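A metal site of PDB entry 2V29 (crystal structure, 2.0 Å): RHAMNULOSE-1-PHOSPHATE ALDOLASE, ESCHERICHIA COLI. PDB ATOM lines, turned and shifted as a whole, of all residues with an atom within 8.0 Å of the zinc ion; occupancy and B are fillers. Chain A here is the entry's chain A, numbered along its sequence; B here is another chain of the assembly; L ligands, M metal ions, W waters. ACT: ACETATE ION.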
ATOM      1  N   TRP A  25     -30.744 -21.522 -23.632  1.00  0.00           N
ATOM      2  CA  TRP A  25     -29.925 -20.325 -23.837  1.00  0.00           C
ATOM      3  C   TRP A  25     -28.858 -20.116 -22.774  1.00  0.00           C
ATOM      4  O   TRP A  25     -28.101 -19.155 -22.847  1.00  0.00           O
ATOM      5  CB  TRP A  25     -30.789 -19.057 -23.820  1.00  0.00           C
ATOM      6  CG  TRP A  25     -31.886 -19.008 -24.858  1.00  0.00           C
ATOM      7  CD1 TRP A  25     -32.025 -19.782 -25.972  1.00  0.00           C
ATOM      8  CD2 TRP A  25     -32.977 -18.081 -24.868  1.00  0.00           C
ATOM      9  NE1 TRP A  25     -33.158 -19.402 -26.678  1.00  0.00           N
ATOM     10  CE2 TRP A  25     -33.761 -18.364 -26.006  1.00  0.00           C
ATOM     11  CE3 TRP A  25     -33.383 -17.059 -23.990  1.00  0.00           C
ATOM     12  CZ2 TRP A  25     -34.916 -17.650 -26.306  1.00  0.00           C
ATOM     13  CZ3 TRP A  25     -34.543 -16.337 -24.292  1.00  0.00           C
ATOM     14  CH2 TRP A  25     -35.282 -16.621 -25.442  1.00  0.00           C
ATOM     15  N   ASP A  26     -28.836 -20.959 -21.746  1.00  0.00           N
ATOM     16  CA  ASP A  26     -28.012 -20.623 -20.577  1.00  0.00           C
ATOM     17  C   ASP A  26     -27.371 -21.855 -19.901  1.00  0.00           C
ATOM     18  O   ASP A  26     -27.557 -22.115 -18.697  1.00  0.00           O
ATOM     19  CB  ASP A  26     -28.817 -19.775 -19.606  1.00  0.00           C
ATOM     20  CG  ASP A  26     -29.156 -18.400 -20.189  1.00  0.00           C
ATOM     21  OD1 ASP A  26     -30.312 -18.183 -20.653  1.00  0.00           O
ATOM     22  OD2 ASP A  26     -28.250 -17.525 -20.235  1.00  0.00           O
ATOM     23  N   GLU A  27     -26.569 -22.570 -20.705  1.00  0.00           N
ATOM     24  CA  GLU A  27     -25.690 -23.671 -20.268  1.00  0.00           C
ATOM     25  C   GLU A  27     -24.760 -23.153 -19.166  1.00  0.00           C
ATOM     26  O   GLU A  27     -24.349 -21.986 -19.190  1.00  0.00           O
ATOM     27  CB  GLU A  27     -24.847 -24.203 -21.459  1.00  0.00           C
ATOM     28  CG  GLU A  27     -23.783 -23.210 -22.038  1.00  0.00           C
ATOM     29  CD  GLU A  27     -24.347 -22.170 -23.002  1.00  0.00           C
ATOM     30  OE1 GLU A  27     -23.541 -21.395 -23.554  1.00  0.00           O
ATOM     31  OE2 GLU A  27     -25.599 -22.113 -23.238  1.00  0.00           O
ATOM     32  N   ASN A  29     -22.865 -21.382 -16.476  1.00  0.00           N
ATOM     33  CA  ASN A  29     -23.079 -20.011 -15.988  1.00  0.00           C
ATOM     34  C   ASN A  29     -23.293 -18.983 -17.117  1.00  0.00           C
ATOM     35  O   ASN A  29     -23.165 -17.766 -16.877  1.00  0.00           O
ATOM     36  CB  ASN A  29     -21.894 -19.580 -15.098  1.00  0.00           C
ATOM     37  CG  ASN A  29     -20.595 -19.501 -15.880  1.00  0.00           C
ATOM     38  OD1 ASN A  29     -20.250 -20.444 -16.586  1.00  0.00           O
ATOM     39  ND2 ASN A  29     -19.882 -18.379 -15.771  1.00  0.00           N
ATOM     40  N   GLY A  30     -23.564 -19.469 -18.333  1.00  0.00           N
ATOM     41  CA  GLY A  30     -23.725 -18.622 -19.505  1.00  0.00           C
ATOM     42  C   GLY A  30     -24.922 -17.734 -19.245  1.00  0.00           C
ATOM     43  O   GLY A  30     -25.991 -18.225 -18.892  1.00  0.00           O
ATOM     44  N   GLY A  31     -24.742 -16.420 -19.345  1.00  0.00           N
ATOM     45  CA  GLY A  31     -25.888 -15.513 -19.215  1.00  0.00           C
ATOM     46  C   GLY A  31     -25.886 -14.732 -17.912  1.00  0.00           C
ATOM     47  O   GLY A  31     -25.332 -15.165 -16.886  1.00  0.00           O
ATOM     48  N   ASN A  32     -26.501 -13.548 -17.942  1.00  0.00           N
ATOM     49  CA  ASN A  32     -26.661 -12.751 -16.728  1.00  0.00           C
ATOM     50  C   ASN A  32     -27.802 -11.759 -16.882  1.00  0.00           C
ATOM     51  O   ASN A  32     -28.228 -11.416 -17.992  1.00  0.00           O
ATOM     52  CB  ASN A  32     -25.337 -12.085 -16.333  1.00  0.00           C
ATOM     53  CG  ASN A  32     -24.407 -11.856 -17.523  1.00  0.00           C
ATOM     54  OD1 ASN A  32     -24.631 -10.971 -18.359  1.00  0.00           O
ATOM     55  ND2 ASN A  32     -23.370 -12.659 -17.604  1.00  0.00           N
ATOM     56  N   GLU A 117     -19.829  -9.226 -14.946  1.00  0.00           N
ATOM     57  CA  GLU A 117     -20.278  -8.241 -15.910  1.00  0.00           C
ATOM     58  C   GLU A 117     -21.192  -7.167 -15.343  1.00  0.00           C
ATOM     59  O   GLU A 117     -21.876  -6.492 -16.094  1.00  0.00           O
ATOM     60  CB  GLU A 117     -20.958  -8.942 -17.084  1.00  0.00           C
ATOM     61  CG  GLU A 117     -20.022  -9.900 -17.749  1.00  0.00           C
ATOM     62  CD  GLU A 117     -20.218  -9.990 -19.233  1.00  0.00           C
ATOM     63  OE1 GLU A 117     -19.287  -9.590 -19.976  1.00  0.00           O
ATOM     64  OE2 GLU A 117     -21.302 -10.471 -19.654  1.00  0.00           O
ATOM     65  N   HIS A 141     -28.553 -10.766 -20.724  1.00  0.00           N
ATOM     66  CA  HIS A 141     -27.610 -11.435 -21.614  1.00  0.00           C
ATOM     67  C   HIS A 141     -27.906 -12.944 -21.618  1.00  0.00           C
ATOM     68  O   HIS A 141     -28.111 -13.523 -20.573  1.00  0.00           O
ATOM     69  CB  HIS A 141     -26.150 -11.136 -21.204  1.00  0.00           C
ATOM     70  CG  HIS A 141     -25.134 -12.024 -21.863  1.00  0.00           C
ATOM     71  ND1 HIS A 141     -24.982 -12.093 -23.235  1.00  0.00           N
ATOM     72  CD2 HIS A 141     -24.201 -12.854 -21.351  1.00  0.00           C
ATOM     73  CE1 HIS A 141     -24.024 -12.947 -23.532  1.00  0.00           C
ATOM     74  NE2 HIS A 141     -23.523 -13.418 -22.400  1.00  0.00           N
ATOM     75  N   CYS A 142     -27.967 -13.552 -22.802  1.00  0.00           N
ATOM     76  CA  CYS A 142     -28.049 -15.005 -22.868  1.00  0.00           C
ATOM     77  C   CYS A 142     -27.392 -15.530 -24.138  1.00  0.00           C
ATOM     78  O   CYS A 142     -27.060 -14.755 -25.051  1.00  0.00           O
ATOM     79  CB  CYS A 142     -29.494 -15.496 -22.808  1.00  0.00           C
ATOM     80  SG  CYS A 142     -30.429 -14.947 -24.170  1.00  0.00           S
ATOM     81  N   HIS A 143     -27.205 -16.835 -24.160  1.00  0.00           N
ATOM     82  CA  HIS A 143     -26.535 -17.486 -25.259  1.00  0.00           C
ATOM     83  C   HIS A 143     -27.566 -18.089 -26.200  1.00  0.00           C
ATOM     84  O   HIS A 143     -27.716 -19.297 -26.306  1.00  0.00           O
ATOM     85  CB  HIS A 143     -25.531 -18.494 -24.727  1.00  0.00           C
ATOM     86  CG  HIS A 143     -24.408 -17.860 -23.962  1.00  0.00           C
ATOM     87  ND1 HIS A 143     -23.475 -18.602 -23.282  1.00  0.00           N
ATOM     88  CD2 HIS A 143     -24.130 -16.558 -23.716  1.00  0.00           C
ATOM     89  CE1 HIS A 143     -22.616 -17.772 -22.697  1.00  0.00           C
ATOM     90  NE2 HIS A 143     -23.004 -16.524 -22.928  1.00  0.00           N
ATOM     91  N   ILE A 148     -26.642 -17.033 -32.198  1.00  0.00           N
ATOM     92  CA  ILE A 148     -25.222 -17.414 -32.230  1.00  0.00           C
ATOM     93  C   ILE A 148     -24.842 -18.097 -33.570  1.00  0.00           C
ATOM     94  O   ILE A 148     -23.901 -17.677 -34.252  1.00  0.00           O
ATOM     95  CB  ILE A 148     -24.850 -18.338 -31.035  1.00  0.00           C
ATOM     96  CG1 ILE A 148     -24.978 -17.577 -29.706  1.00  0.00           C
ATOM     97  CG2 ILE A 148     -23.372 -18.883 -31.198  1.00  0.00           C
ATOM     98  CD1 ILE A 148     -25.034 -18.507 -28.429  1.00  0.00           C
ATOM     99  N   PRO A 188     -14.633 -11.255 -23.713  1.00  0.00           N
ATOM    100  CA  PRO A 188     -15.710 -10.927 -22.773  1.00  0.00           C
ATOM    101  C   PRO A 188     -15.211 -10.505 -21.380  1.00  0.00           C
ATOM    102  O   PRO A 188     -14.058 -10.805 -21.008  1.00  0.00           O
ATOM    103  CB  PRO A 188     -16.494 -12.239 -22.641  1.00  0.00           C
ATOM    104  CG  PRO A 188     -15.869 -13.208 -23.557  1.00  0.00           C
ATOM    105  CD  PRO A 188     -14.534 -12.693 -23.981  1.00  0.00           C
ATOM    106  N   GLY A 189     -16.072  -9.845 -20.618  1.00  0.00           N
ATOM    107  CA  GLY A 189     -15.730  -9.382 -19.278  1.00  0.00           C
ATOM    108  C   GLY A 189     -14.739  -8.225 -19.223  1.00  0.00           C
ATOM    109  O   GLY A 189     -14.304  -7.863 -18.119  1.00  0.00           O
ATOM    110  N   TRP A 209     -23.101 -10.171 -29.898  1.00  0.00           N
ATOM    111  CA  TRP A 209     -21.698 -10.467 -29.694  1.00  0.00           C
ATOM    112  C   TRP A 209     -21.439 -11.720 -30.513  1.00  0.00           C
ATOM    113  O   TRP A 209     -21.820 -12.787 -30.105  1.00  0.00           O
ATOM    114  CB  TRP A 209     -21.501 -10.808 -28.205  1.00  0.00           C
ATOM    115  CG  TRP A 209     -21.508  -9.614 -27.288  1.00  0.00           C
ATOM    116  CD1 TRP A 209     -21.760  -8.295 -27.630  1.00  0.00           C
ATOM    117  CD2 TRP A 209     -21.275  -9.644 -25.899  1.00  0.00           C
ATOM    118  NE1 TRP A 209     -21.700  -7.505 -26.509  1.00  0.00           N
ATOM    119  CE2 TRP A 209     -21.409  -8.303 -25.428  1.00  0.00           C
ATOM    120  CE3 TRP A 209     -20.962 -10.659 -24.989  1.00  0.00           C
ATOM    121  CZ2 TRP A 209     -21.201  -7.959 -24.078  1.00  0.00           C
ATOM    122  CZ3 TRP A 209     -20.756 -10.333 -23.663  1.00  0.00           C
ATOM    123  CH2 TRP A 209     -20.870  -8.974 -23.204  1.00  0.00           C
ATOM    124  N   PHE A 211     -20.367 -15.115 -32.212  1.00  0.00           N
ATOM    125  CA  PHE A 211     -19.790 -16.336 -31.634  1.00  0.00           C
ATOM    126  C   PHE A 211     -20.000 -16.452 -30.128  1.00  0.00           C
ATOM    127  O   PHE A 211     -19.276 -17.193 -29.448  1.00  0.00           O
ATOM    128  CB  PHE A 211     -18.260 -16.449 -31.964  1.00  0.00           C
ATOM    129  CG  PHE A 211     -17.878 -15.913 -33.336  1.00  0.00           C
ATOM    130  CD1 PHE A 211     -16.757 -15.072 -33.480  1.00  0.00           C
ATOM    131  CD2 PHE A 211     -18.644 -16.230 -34.466  1.00  0.00           C
ATOM    132  CE1 PHE A 211     -16.431 -14.560 -34.734  1.00  0.00           C
ATOM    133  CE2 PHE A 211     -18.316 -15.726 -35.709  1.00  0.00           C
ATOM    134  CZ  PHE A 211     -17.188 -14.881 -35.849  1.00  0.00           C
ATOM    135  N   HIS A 212     -20.942 -15.691 -29.580  1.00  0.00           N
ATOM    136  CA  HIS A 212     -21.104 -15.665 -28.125  1.00  0.00           C
ATOM    137  C   HIS A 212     -22.579 -15.568 -27.702  1.00  0.00           C
ATOM    138  O   HIS A 212     -23.131 -16.483 -27.052  1.00  0.00           O
ATOM    139  CB  HIS A 212     -20.273 -14.484 -27.570  1.00  0.00           C
ATOM    140  CG  HIS A 212     -20.302 -14.353 -26.082  1.00  0.00           C
ATOM    141  ND1 HIS A 212     -19.352 -13.630 -25.377  1.00  0.00           N
ATOM    142  CD2 HIS A 212     -21.171 -14.826 -25.155  1.00  0.00           C
ATOM    143  CE1 HIS A 212     -19.634 -13.690 -24.093  1.00  0.00           C
ATOM    144  NE2 HIS A 212     -20.734 -14.384 -23.926  1.00  0.00           N
ATOM    145  N   GLY A 213     -23.249 -14.461 -28.016  1.00  0.00           N
ATOM    146  CA  GLY A 213     -24.649 -14.334 -27.545  1.00  0.00           C
ATOM    147  C   GLY A 213     -25.246 -12.946 -27.785  1.00  0.00           C
ATOM    148  O   GLY A 213     -24.759 -12.175 -28.636  1.00  0.00           O
ATOM    149  N   VAL A 214     -26.313 -12.667 -27.063  1.00  0.00           N
ATOM    150  CA  VAL A 214     -27.128 -11.467 -27.289  1.00  0.00           C
ATOM    151  C   VAL A 214     -27.288 -10.712 -25.965  1.00  0.00           C
ATOM    152  O   VAL A 214     -27.198 -11.316 -24.877  1.00  0.00           O
ATOM    153  CB  VAL A 214     -28.508 -11.805 -27.939  1.00  0.00           C
ATOM    154  CG1 VAL A 214     -29.390 -12.642 -26.992  1.00  0.00           C
ATOM    155  CG2 VAL A 214     -29.264 -10.543 -28.424  1.00  0.00           C
ATOM    156  N   PHE A 215     -27.504  -9.413 -26.090  1.00  0.00           N
ATOM    157  CA  PHE A 215     -27.811  -8.473 -25.010  1.00  0.00           C
ATOM    158  C   PHE A 215     -29.046  -7.672 -25.347  1.00  0.00           C
ATOM    159  O   PHE A 215     -29.125  -7.072 -26.429  1.00  0.00           O
ATOM    160  CB  PHE A 215     -26.679  -7.465 -24.879  1.00  0.00           C
ATOM    161  CG  PHE A 215     -25.728  -7.798 -23.816  1.00  0.00           C
ATOM    162  CD1 PHE A 215     -24.771  -8.772 -24.027  1.00  0.00           C
ATOM    163  CD2 PHE A 215     -25.804  -7.188 -22.598  1.00  0.00           C
ATOM    164  CE1 PHE A 215     -23.905  -9.104 -23.005  1.00  0.00           C
ATOM    165  CE2 PHE A 215     -24.948  -7.503 -21.580  1.00  0.00           C
ATOM    166  CZ  PHE A 215     -23.999  -8.476 -21.773  1.00  0.00           C
ATOM    167  N   THR B 170     -17.853 -18.921 -27.516  1.00  0.00           N
ATOM    168  CA  THR B 170     -16.677 -18.206 -26.969  1.00  0.00           C
ATOM    169  C   THR B 170     -16.155 -18.792 -25.640  1.00  0.00           C
ATOM    170  O   THR B 170     -14.952 -18.949 -25.462  1.00  0.00           O
ATOM    171  CB  THR B 170     -16.946 -16.664 -26.893  1.00  0.00           C
ATOM    172  OG1 THR B 170     -17.049 -16.183 -28.211  1.00  0.00           O
ATOM    173  CG2 THR B 170     -15.762 -15.887 -26.208  1.00  0.00           C
ATOM    174  N   GLU B 171     -17.080 -19.176 -24.750  1.00  0.00           N
ATOM    175  CA  GLU B 171     -16.717 -19.726 -23.441  1.00  0.00           C
ATOM    176  C   GLU B 171     -15.974 -21.063 -23.463  1.00  0.00           C
ATOM    177  O   GLU B 171     -15.358 -21.397 -22.461  1.00  0.00           O
ATOM    178  CB  GLU B 171     -17.982 -19.945 -22.590  1.00  0.00           C
ATOM    179  CG  GLU B 171     -18.794 -21.124 -23.136  1.00  0.00           C
ATOM    180  CD  GLU B 171     -20.278 -21.123 -22.797  1.00  0.00           C
ATOM    181  OE1 GLU B 171     -20.723 -20.404 -21.877  1.00  0.00           O
ATOM    182  OE2 GLU B 171     -21.002 -21.877 -23.470  1.00  0.00           O
HETATM  183  C   ACT L   1     -21.255 -15.391 -19.943  1.00  0.00           C
HETATM  184  O   ACT L   1     -22.443 -15.119 -20.022  1.00  0.00           O
HETATM  185  OXT ACT L   1     -20.598 -15.499 -20.994  1.00  0.00           O
HETATM  186  CH3 ACT L   1     -20.602 -15.586 -18.599  1.00  0.00           C
HETATM  187 ZN    ZN M   1     -21.952 -14.799 -22.322  1.00  0.00          ZN
HETATM  188  O   HOH W   1     -20.312 -12.839 -20.852  1.00  0.00           O
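The nearest printed residue that does not touch the zinc ion is Gly 31 (4.4 Å).
The zinc ion is bound by an oxygen (OXT) of the ligand (2.0 Å), a ring nitrogen (NE2) of His 212 (2.1 Å), a ring nitrogen (NE2) of His 141 (2.1 Å), a ring nitrogen (NE2) of His 143 (2.1 Å) and an oxygen (O) of the ligand (2.4 Å).
The zinc ion has five donor atoms within binding distance.
ND1 of His 143 lies within hydrogen-bond range of OE1 of Glu 27, at 2.8 Å.
The backbone NH (N) of His 141 sits at hydrogen-bond distance from the backbone carbonyl oxygen (O) of Asn 32.
The backbone NH (N) of His 143 is in hydrogen-bond range of the backbone carbonyl oxygen (O) of Trp 25 (2.8 Å).
O of Val 214 lies within hydrogen-bond range of ND1 of His 141 (2.9 Å).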
